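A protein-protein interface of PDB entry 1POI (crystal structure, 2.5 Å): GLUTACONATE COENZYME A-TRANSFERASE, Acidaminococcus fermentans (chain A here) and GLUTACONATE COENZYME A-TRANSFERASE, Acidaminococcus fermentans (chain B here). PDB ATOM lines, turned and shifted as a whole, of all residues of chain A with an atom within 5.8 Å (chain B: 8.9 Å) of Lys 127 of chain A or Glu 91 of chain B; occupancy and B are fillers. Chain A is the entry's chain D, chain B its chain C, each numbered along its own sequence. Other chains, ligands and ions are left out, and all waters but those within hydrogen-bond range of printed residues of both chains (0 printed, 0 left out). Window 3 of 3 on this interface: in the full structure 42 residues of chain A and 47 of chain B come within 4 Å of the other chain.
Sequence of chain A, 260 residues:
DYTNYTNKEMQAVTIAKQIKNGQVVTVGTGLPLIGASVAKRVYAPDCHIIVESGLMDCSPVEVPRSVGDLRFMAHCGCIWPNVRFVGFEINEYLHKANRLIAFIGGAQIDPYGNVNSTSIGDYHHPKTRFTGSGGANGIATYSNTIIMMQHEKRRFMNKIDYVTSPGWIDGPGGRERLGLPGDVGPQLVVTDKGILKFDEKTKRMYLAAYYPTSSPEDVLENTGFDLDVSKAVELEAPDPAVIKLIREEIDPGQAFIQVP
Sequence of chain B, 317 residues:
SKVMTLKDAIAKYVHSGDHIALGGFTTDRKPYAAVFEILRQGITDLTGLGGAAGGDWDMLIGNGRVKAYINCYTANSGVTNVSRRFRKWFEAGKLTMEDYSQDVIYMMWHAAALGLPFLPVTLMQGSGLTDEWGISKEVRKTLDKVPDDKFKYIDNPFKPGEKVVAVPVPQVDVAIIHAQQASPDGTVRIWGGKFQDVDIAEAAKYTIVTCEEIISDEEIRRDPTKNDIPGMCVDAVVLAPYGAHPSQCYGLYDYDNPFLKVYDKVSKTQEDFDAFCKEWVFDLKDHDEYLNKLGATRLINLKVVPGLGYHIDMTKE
The guanidinium group of Arg 87 of chain B lies within hydrogen-bond range of the backbone carbonyl oxygen of Arg 129 of chain A (2.9 Å).
The backbone NH (N) of Arg 129 of chain A sits at hydrogen-bond distance from the side-chain carboxylate (OE2) of Glu 91 of chain B, 2.8 Å away.
The side-chain carboxylate (OE2) of Glu 91 of chain B lies within salt-bridge range of the guanidinium group (NE) of Arg 87 of chain B (3.4 Å).
O of Ile 120 of chain A is in hydrogen-bond range of N of Lys 127 of chain A, at 2.8 Å.
The backbone NH (N) of Ile 120 of chain A is in hydrogen-bond range of the backbone carbonyl oxygen (O) of Thr 128 of chain A (2.9 Å).
Of the printed residues of chain B, Lys 127 of chain A touches Glu 91 (3.7 Å).
Of chain A, only Lys 127, Thr 128 and Arg 129 come within 4 Å of Glu 91 of chain B.
Of chain B, only Glu 91 (3.5 Å) comes within 4 Å of Thr 128 of chain A.
Printed residues of chain B within 4 Å of Phe 130 of chain A: Val 82 (3.9 Å) and Phe 86 (3.9 Å).
Printed residues of chain A within 4 Å of Val 82 of chain B: Phe 130 (3.9 Å).
Of the printed residues of chain B, Arg 129 of chain A touches Arg 87, Phe 90, Glu 91 and Met 97.
Of the printed residues of chain A, Phe 86 of chain B touches Phe 130.
Of the 9 printed residues of chain A, 5 touch a printed residue of chain B.
Printed residues of chain A that touch a printed residue of chain B: Pro 126, Lys 127, Thr 128, Arg 129 and Phe 130.
Hydrophobic or aromatic side chains of chain A within 4 Å of the printed part of chain B: Pro 126.
Among the printed residues, no Asp or Glu carboxylate lies within 4 Å of a Lys or Arg side-chain nitrogen of the other chain.
Pro 126 of chain A touches Phe 90 of chain B.
O of Lys 127 of chain A touches OE2 of Glu 91 of chain B (3.7 Å).
Thr 128 of chain A touches Glu 91 of chain B (CA to OE2, 3.5 Å).
Phe 90 of chain B touches Arg 129 of chain A.
Arg 129 of chain A touches Met 97 of chain B (NH1 to CE, 2.8 Å).
CG1 of Val 82 of chain B touches C of Phe 130 of chain A (3.9 Å).
Phe 130 of chain A touches Phe 86 of chain B.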
ATOM      1  N   ILE A 120       3.817 -21.074   5.942  1.00  0.00           N
ATOM      2  CA  ILE A 120       4.199 -19.789   6.547  1.00  0.00           C
ATOM      3  C   ILE A 120       5.709 -19.627   6.563  1.00  0.00           C
ATOM      4  O   ILE A 120       6.407 -20.458   7.141  1.00  0.00           O
ATOM      5  CB  ILE A 120       3.661 -19.716   7.966  1.00  0.00           C
ATOM      6  CG1 ILE A 120       2.156 -19.455   7.898  1.00  0.00           C
ATOM      7  CG2 ILE A 120       4.417 -18.702   8.770  1.00  0.00           C
ATOM      8  CD1 ILE A 120       1.488 -19.237   9.234  1.00  0.00           C
ATOM      9  N   GLY A 121       6.195 -18.546   5.956  1.00  0.00           N
ATOM     10  CA  GLY A 121       7.624 -18.310   5.860  1.00  0.00           C
ATOM     11  C   GLY A 121       8.144 -18.774   4.503  1.00  0.00           C
ATOM     12  O   GLY A 121       7.355 -19.018   3.594  1.00  0.00           O
ATOM     13  N   ASP A 122       9.456 -18.902   4.344  1.00  0.00           N
ATOM     14  CA  ASP A 122      10.001 -19.355   3.074  1.00  0.00           C
ATOM     15  C   ASP A 122       9.360 -20.679   2.649  1.00  0.00           C
ATOM     16  O   ASP A 122       9.619 -21.708   3.247  1.00  0.00           O
ATOM     17  CB  ASP A 122      11.513 -19.548   3.178  1.00  0.00           C
ATOM     18  CG  ASP A 122      12.131 -20.126   1.899  1.00  0.00           C
ATOM     19  OD1 ASP A 122      11.458 -20.133   0.835  1.00  0.00           O
ATOM     20  OD2 ASP A 122      13.301 -20.579   1.955  1.00  0.00           O
ATOM     21  N   HIS A 125      11.466 -23.804   2.666  1.00  0.00           N
ATOM     22  CA  HIS A 125      11.991 -24.188   3.982  1.00  0.00           C
ATOM     23  C   HIS A 125      11.084 -23.431   4.931  1.00  0.00           C
ATOM     24  O   HIS A 125      11.511 -22.503   5.609  1.00  0.00           O
ATOM     25  CB  HIS A 125      13.429 -23.711   4.170  1.00  0.00           C
ATOM     26  CG  HIS A 125      14.354 -24.127   3.074  1.00  0.00           C
ATOM     27  ND1 HIS A 125      14.640 -23.314   1.998  1.00  0.00           N
ATOM     28  CD2 HIS A 125      15.067 -25.262   2.887  1.00  0.00           C
ATOM     29  CE1 HIS A 125      15.492 -23.928   1.193  1.00  0.00           C
ATOM     30  NE2 HIS A 125      15.766 -25.112   1.710  1.00  0.00           N
ATOM     31  N   PRO A 126       9.808 -23.810   4.970  1.00  0.00           N
ATOM     32  CA  PRO A 126       8.795 -23.176   5.810  1.00  0.00           C
ATOM     33  C   PRO A 126       9.001 -23.203   7.309  1.00  0.00           C
ATOM     34  O   PRO A 126       9.713 -24.047   7.851  1.00  0.00           O
ATOM     35  CB  PRO A 126       7.528 -23.929   5.417  1.00  0.00           C
ATOM     36  CG  PRO A 126       8.055 -25.316   5.143  1.00  0.00           C
ATOM     37  CD  PRO A 126       9.252 -24.997   4.298  1.00  0.00           C
ATOM     38  N   LYS A 127       8.339 -22.266   7.968  1.00  0.00           N
ATOM     39  CA  LYS A 127       8.379 -22.160   9.407  1.00  0.00           C
ATOM     40  C   LYS A 127       7.284 -23.125   9.827  1.00  0.00           C
ATOM     41  O   LYS A 127       7.479 -23.962  10.706  1.00  0.00           O
ATOM     42  CB  LYS A 127       8.052 -20.722   9.823  1.00  0.00           C
ATOM     43  CG  LYS A 127       8.031 -20.462  11.315  1.00  0.00           C
ATOM     44  CD  LYS A 127       8.303 -18.982  11.638  1.00  0.00           C
ATOM     45  CE  LYS A 127       7.239 -18.023  11.067  1.00  0.00           C
ATOM     46  NZ  LYS A 127       7.748 -17.126   9.957  1.00  0.00           N
ATOM     47  N   THR A 128       6.155 -23.046   9.127  1.00  0.00           N
ATOM     48  CA  THR A 128       5.015 -23.917   9.387  1.00  0.00           C
ATOM     49  C   THR A 128       4.448 -24.434   8.062  1.00  0.00           C
ATOM     50  O   THR A 128       4.070 -23.654   7.181  1.00  0.00           O
ATOM     51  CB  THR A 128       3.914 -23.192  10.167  1.00  0.00           C
ATOM     52  OG1 THR A 128       4.478 -22.603  11.351  1.00  0.00           O
ATOM     53  CG2 THR A 128       2.813 -24.180  10.547  1.00  0.00           C
ATOM     54  N   ARG A 129       4.483 -25.752   7.903  1.00  0.00           N
ATOM     55  CA  ARG A 129       3.999 -26.410   6.704  1.00  0.00           C
ATOM     56  C   ARG A 129       2.592 -26.901   6.998  1.00  0.00           C
ATOM     57  O   ARG A 129       2.322 -27.398   8.091  1.00  0.00           O
ATOM     58  CB  ARG A 129       4.915 -27.570   6.344  1.00  0.00           C
ATOM     59  CG  ARG A 129       4.463 -28.359   5.143  1.00  0.00           C
ATOM     60  CD  ARG A 129       4.345 -27.506   3.883  1.00  0.00           C
ATOM     61  NE  ARG A 129       3.141 -27.871   3.152  1.00  0.00           N
ATOM     62  CZ  ARG A 129       3.040 -27.955   1.831  1.00  0.00           C
ATOM     63  NH1 ARG A 129       4.083 -27.684   1.049  1.00  0.00           N
ATOM     64  NH2 ARG A 129       1.906 -28.381   1.298  1.00  0.00           N
ATOM     65  N   PHE A 130       1.676 -26.648   6.072  1.00  0.00           N
ATOM     66  CA  PHE A 130       0.288 -27.057   6.236  1.00  0.00           C
ATOM     67  C   PHE A 130       0.028 -28.154   5.225  1.00  0.00           C
ATOM     68  O   PHE A 130       0.949 -28.621   4.570  1.00  0.00           O
ATOM     69  CB  PHE A 130      -0.665 -25.895   5.979  1.00  0.00           C
ATOM     70  CG  PHE A 130      -0.382 -24.674   6.798  1.00  0.00           C
ATOM     71  CD1 PHE A 130      -0.667 -24.647   8.152  1.00  0.00           C
ATOM     72  CD2 PHE A 130       0.155 -23.528   6.199  1.00  0.00           C
ATOM     73  CE1 PHE A 130      -0.422 -23.497   8.900  1.00  0.00           C
ATOM     74  CE2 PHE A 130       0.408 -22.367   6.944  1.00  0.00           C
ATOM     75  CZ  PHE A 130       0.117 -22.359   8.294  1.00  0.00           C
ATOM     76  N   VAL B  82      -2.999 -32.118   9.867  1.00  0.00           N
ATOM     77  CA  VAL B  82      -1.836 -32.110   8.995  1.00  0.00           C
ATOM     78  C   VAL B  82      -1.044 -33.323   9.404  1.00  0.00           C
ATOM     79  O   VAL B  82      -0.764 -33.518  10.582  1.00  0.00           O
ATOM     80  CB  VAL B  82      -0.922 -30.870   9.156  1.00  0.00           C
ATOM     81  CG1 VAL B  82       0.129 -30.864   8.033  1.00  0.00           C
ATOM     82  CG2 VAL B  82      -1.734 -29.588   9.151  1.00  0.00           C
ATOM     83  N   SER B  83      -0.740 -34.175   8.441  1.00  0.00           N
ATOM     84  CA  SER B  83       0.023 -35.358   8.739  1.00  0.00           C
ATOM     85  C   SER B  83       1.354 -34.952   9.327  1.00  0.00           C
ATOM     86  O   SER B  83       2.286 -34.537   8.629  1.00  0.00           O
ATOM     87  CB  SER B  83       0.165 -36.224   7.499  1.00  0.00           C
ATOM     88  OG  SER B  83      -1.070 -36.880   7.237  1.00  0.00           O
ATOM     89  N   ARG B  84       1.392 -35.050  10.647  1.00  0.00           N
ATOM     90  CA  ARG B  84       2.546 -34.695  11.451  1.00  0.00           C
ATOM     91  C   ARG B  84       3.926 -35.126  10.942  1.00  0.00           C
ATOM     92  O   ARG B  84       4.836 -34.304  10.900  1.00  0.00           O
ATOM     93  CB  ARG B  84       2.312 -35.166  12.865  1.00  0.00           C
ATOM     94  CG  ARG B  84       1.015 -34.659  13.409  1.00  0.00           C
ATOM     95  CD  ARG B  84       0.854 -35.155  14.813  1.00  0.00           C
ATOM     96  NE  ARG B  84      -0.374 -34.726  15.468  1.00  0.00           N
ATOM     97  CZ  ARG B  84      -0.594 -33.495  15.917  1.00  0.00           C
ATOM     98  NH1 ARG B  84       0.329 -32.553  15.746  1.00  0.00           N
ATOM     99  NH2 ARG B  84      -1.669 -33.247  16.671  1.00  0.00           N
ATOM    100  N   ARG B  85       4.074 -36.381  10.538  1.00  0.00           N
ATOM    101  CA  ARG B  85       5.342 -36.893  10.019  1.00  0.00           C
ATOM    102  C   ARG B  85       5.666 -36.224   8.667  1.00  0.00           C
ATOM    103  O   ARG B  85       6.826 -35.937   8.349  1.00  0.00           O
ATOM    104  CB  ARG B  85       5.249 -38.427   9.834  1.00  0.00           C
ATOM    105  CG  ARG B  85       6.316 -39.266  10.528  1.00  0.00           C
ATOM    106  CD  ARG B  85       6.356 -38.982  12.016  1.00  0.00           C
ATOM    107  NE  ARG B  85       7.604 -38.308  12.334  1.00  0.00           N
ATOM    108  CZ  ARG B  85       7.737 -37.294  13.187  1.00  0.00           C
ATOM    109  NH1 ARG B  85       6.691 -36.811  13.842  1.00  0.00           N
ATOM    110  NH2 ARG B  85       8.923 -36.719  13.341  1.00  0.00           N
ATOM    111  N   PHE B  86       4.628 -35.974   7.880  1.00  0.00           N
ATOM    112  CA  PHE B  86       4.773 -35.355   6.567  1.00  0.00           C
ATOM    113  C   PHE B  86       5.298 -33.929   6.745  1.00  0.00           C
ATOM    114  O   PHE B  86       6.303 -33.557   6.136  1.00  0.00           O
ATOM    115  CB  PHE B  86       3.413 -35.400   5.825  1.00  0.00           C
ATOM    116  CG  PHE B  86       3.212 -34.304   4.795  1.00  0.00           C
ATOM    117  CD1 PHE B  86       3.909 -34.314   3.588  1.00  0.00           C
ATOM    118  CD2 PHE B  86       2.300 -33.277   5.030  1.00  0.00           C
ATOM    119  CE1 PHE B  86       3.695 -33.311   2.627  1.00  0.00           C
ATOM    120  CE2 PHE B  86       2.087 -32.282   4.088  1.00  0.00           C
ATOM    121  CZ  PHE B  86       2.789 -32.301   2.883  1.00  0.00           C
ATOM    122  N   ARG B  87       4.659 -33.164   7.629  1.00  0.00           N
ATOM    123  CA  ARG B  87       5.088 -31.795   7.870  1.00  0.00           C
ATOM    124  C   ARG B  87       6.484 -31.722   8.506  1.00  0.00           C
ATOM    125  O   ARG B  87       7.351 -31.007   7.997  1.00  0.00           O
ATOM    126  CB  ARG B  87       4.058 -31.013   8.679  1.00  0.00           C
ATOM    127  CG  ARG B  87       4.021 -31.315  10.130  1.00  0.00           C
ATOM    128  CD  ARG B  87       4.236 -30.036  10.917  1.00  0.00           C
ATOM    129  NE  ARG B  87       3.244 -29.030  10.576  1.00  0.00           N
ATOM    130  CZ  ARG B  87       2.041 -28.951  11.132  1.00  0.00           C
ATOM    131  NH1 ARG B  87       1.690 -29.820  12.075  1.00  0.00           N
ATOM    132  NH2 ARG B  87       1.161 -28.053  10.684  1.00  0.00           N
ATOM    133  N   LYS B  88       6.727 -32.482   9.572  1.00  0.00           N
ATOM    134  CA  LYS B  88       8.040 -32.466  10.203  1.00  0.00           C
ATOM    135  C   LYS B  88       9.119 -32.827   9.198  1.00  0.00           C
ATOM    136  O   LYS B  88      10.078 -32.079   9.013  1.00  0.00           O
ATOM    137  CB  LYS B  88       8.109 -33.455  11.356  1.00  0.00           C
ATOM    138  CG  LYS B  88       7.190 -33.126  12.486  1.00  0.00           C
ATOM    139  CD  LYS B  88       7.451 -31.725  12.999  1.00  0.00           C
ATOM    140  CE  LYS B  88       6.543 -31.440  14.169  1.00  0.00           C
ATOM    141  NZ  LYS B  88       5.129 -31.728  13.815  1.00  0.00           N
ATOM    142  N   TRP B  89       8.940 -33.947   8.515  1.00  0.00           N
ATOM    143  CA  TRP B  89       9.921 -34.399   7.546  1.00  0.00           C
ATOM    144  C   TRP B  89      10.208 -33.407   6.420  1.00  0.00           C
ATOM    145  O   TRP B  89      11.296 -33.420   5.835  1.00  0.00           O
ATOM    146  CB  TRP B  89       9.489 -35.744   6.974  1.00  0.00           C
ATOM    147  CG  TRP B  89       9.964 -36.915   7.792  1.00  0.00           C
ATOM    148  CD1 TRP B  89       9.628 -37.216   9.090  1.00  0.00           C
ATOM    149  CD2 TRP B  89      10.919 -37.890   7.391  1.00  0.00           C
ATOM    150  NE1 TRP B  89      10.341 -38.319   9.519  1.00  0.00           N
ATOM    151  CE2 TRP B  89      11.139 -38.745   8.490  1.00  0.00           C
ATOM    152  CE3 TRP B  89      11.618 -38.118   6.209  1.00  0.00           C
ATOM    153  CZ2 TRP B  89      12.037 -39.805   8.437  1.00  0.00           C
ATOM    154  CZ3 TRP B  89      12.510 -39.165   6.150  1.00  0.00           C
ATOM    155  CH2 TRP B  89      12.715 -39.999   7.257  1.00  0.00           C
ATOM    156  N   PHE B  90       9.227 -32.565   6.102  1.00  0.00           N
ATOM    157  CA  PHE B  90       9.379 -31.569   5.045  1.00  0.00           C
ATOM    158  C   PHE B  90      10.068 -30.320   5.577  1.00  0.00           C
ATOM    159  O   PHE B  90      10.988 -29.793   4.955  1.00  0.00           O
ATOM    160  CB  PHE B  90       8.018 -31.196   4.445  1.00  0.00           C
ATOM    161  CG  PHE B  90       8.117 -30.189   3.338  1.00  0.00           C
ATOM    162  CD1 PHE B  90       8.757 -30.519   2.136  1.00  0.00           C
ATOM    163  CD2 PHE B  90       7.675 -28.881   3.530  1.00  0.00           C
ATOM    164  CE1 PHE B  90       8.969 -29.546   1.143  1.00  0.00           C
ATOM    165  CE2 PHE B  90       7.883 -27.911   2.549  1.00  0.00           C
ATOM    166  CZ  PHE B  90       8.535 -28.244   1.349  1.00  0.00           C
ATOM    167  N   GLU B  91       9.599 -29.842   6.724  1.00  0.00           N
ATOM    168  CA  GLU B  91      10.161 -28.661   7.368  1.00  0.00           C
ATOM    169  C   GLU B  91      11.642 -28.902   7.666  1.00  0.00           C
ATOM    170  O   GLU B  91      12.467 -28.017   7.444  1.00  0.00           O
ATOM    171  CB  GLU B  91       9.397 -28.324   8.654  1.00  0.00           C
ATOM    172  CG  GLU B  91       7.930 -28.023   8.424  1.00  0.00           C
ATOM    173  CD  GLU B  91       7.145 -27.841   9.717  1.00  0.00           C
ATOM    174  OE1 GLU B  91       7.594 -28.276  10.796  1.00  0.00           O
ATOM    175  OE2 GLU B  91       6.047 -27.267   9.674  1.00  0.00           O
ATOM    176  N   ALA B  92      11.980 -30.107   8.122  1.00  0.00           N
ATOM    177  CA  ALA B  92      13.365 -30.465   8.432  1.00  0.00           C
ATOM    178  C   ALA B  92      14.192 -30.605   7.151  1.00  0.00           C
ATOM    179  O   ALA B  92      15.412 -30.818   7.197  1.00  0.00           O
ATOM    180  CB  ALA B  92      13.406 -31.750   9.242  1.00  0.00           C
ATOM    181  N   GLY B  93      13.513 -30.537   6.010  1.00  0.00           N
ATOM    182  CA  GLY B  93      14.181 -30.620   4.728  1.00  0.00           C
ATOM    183  C   GLY B  93      14.585 -32.002   4.284  1.00  0.00           C
ATOM    184  O   GLY B  93      15.530 -32.153   3.507  1.00  0.00           O
ATOM    185  N   LYS B  94      13.888 -33.017   4.774  1.00  0.00           N
ATOM    186  CA  LYS B  94      14.204 -34.380   4.384  1.00  0.00           C
ATOM    187  C   LYS B  94      13.324 -34.846   3.230  1.00  0.00           C
ATOM    188  O   LYS B  94      13.779 -35.583   2.359  1.00  0.00           O
ATOM    189  CB  LYS B  94      14.086 -35.311   5.581  1.00  0.00           C
ATOM    190  CG  LYS B  94      15.144 -35.045   6.621  1.00  0.00           C
ATOM    191  CD  LYS B  94      15.054 -35.997   7.798  1.00  0.00           C
ATOM    192  CE  LYS B  94      13.866 -35.656   8.685  1.00  0.00           C
ATOM    193  NZ  LYS B  94      13.859 -36.501   9.925  1.00  0.00           N
ATOM    194  N   LEU B  95      12.090 -34.343   3.183  1.00  0.00           N
ATOM    195  CA  LEU B  95      11.121 -34.709   2.141  1.00  0.00           C
ATOM    196  C   LEU B  95      11.133 -33.812   0.894  1.00  0.00           C
ATOM    197  O   LEU B  95      10.771 -32.634   0.970  1.00  0.00           O
ATOM    198  CB  LEU B  95       9.702 -34.688   2.740  1.00  0.00           C
ATOM    199  CG  LEU B  95       8.557 -35.614   2.306  1.00  0.00           C
ATOM    200  CD1 LEU B  95       7.194 -34.947   2.624  1.00  0.00           C
ATOM    201  CD2 LEU B  95       8.668 -35.932   0.843  1.00  0.00           C
ATOM    202  N   THR B  96      11.569 -34.379  -0.232  1.00  0.00           N
ATOM    203  CA  THR B  96      11.573 -33.722  -1.544  1.00  0.00           C
ATOM    204  C   THR B  96      10.094 -33.774  -1.957  1.00  0.00           C
ATOM    205  O   THR B  96       9.518 -34.865  -2.084  1.00  0.00           O
ATOM    206  CB  THR B  96      12.360 -34.554  -2.550  1.00  0.00           C
ATOM    207  OG1 THR B  96      13.760 -34.342  -2.348  1.00  0.00           O
ATOM    208  CG2 THR B  96      11.963 -34.211  -3.974  1.00  0.00           C
ATOM    209  N   MET B  97       9.504 -32.625  -2.256  1.00  0.00           N
ATOM    210  CA  MET B  97       8.079 -32.596  -2.545  1.00  0.00           C
ATOM    211  C   MET B  97       7.642 -31.507  -3.546  1.00  0.00           C
ATOM    212  O   MET B  97       8.356 -30.527  -3.771  1.00  0.00           O
ATOM    213  CB  MET B  97       7.357 -32.432  -1.193  1.00  0.00           C
ATOM    214  CG  MET B  97       5.897 -32.068  -1.247  1.00  0.00           C
ATOM    215  SD  MET B  97       5.253 -31.982   0.417  1.00  0.00           S
ATOM    216  CE  MET B  97       5.043 -30.298   0.581  1.00  0.00           C
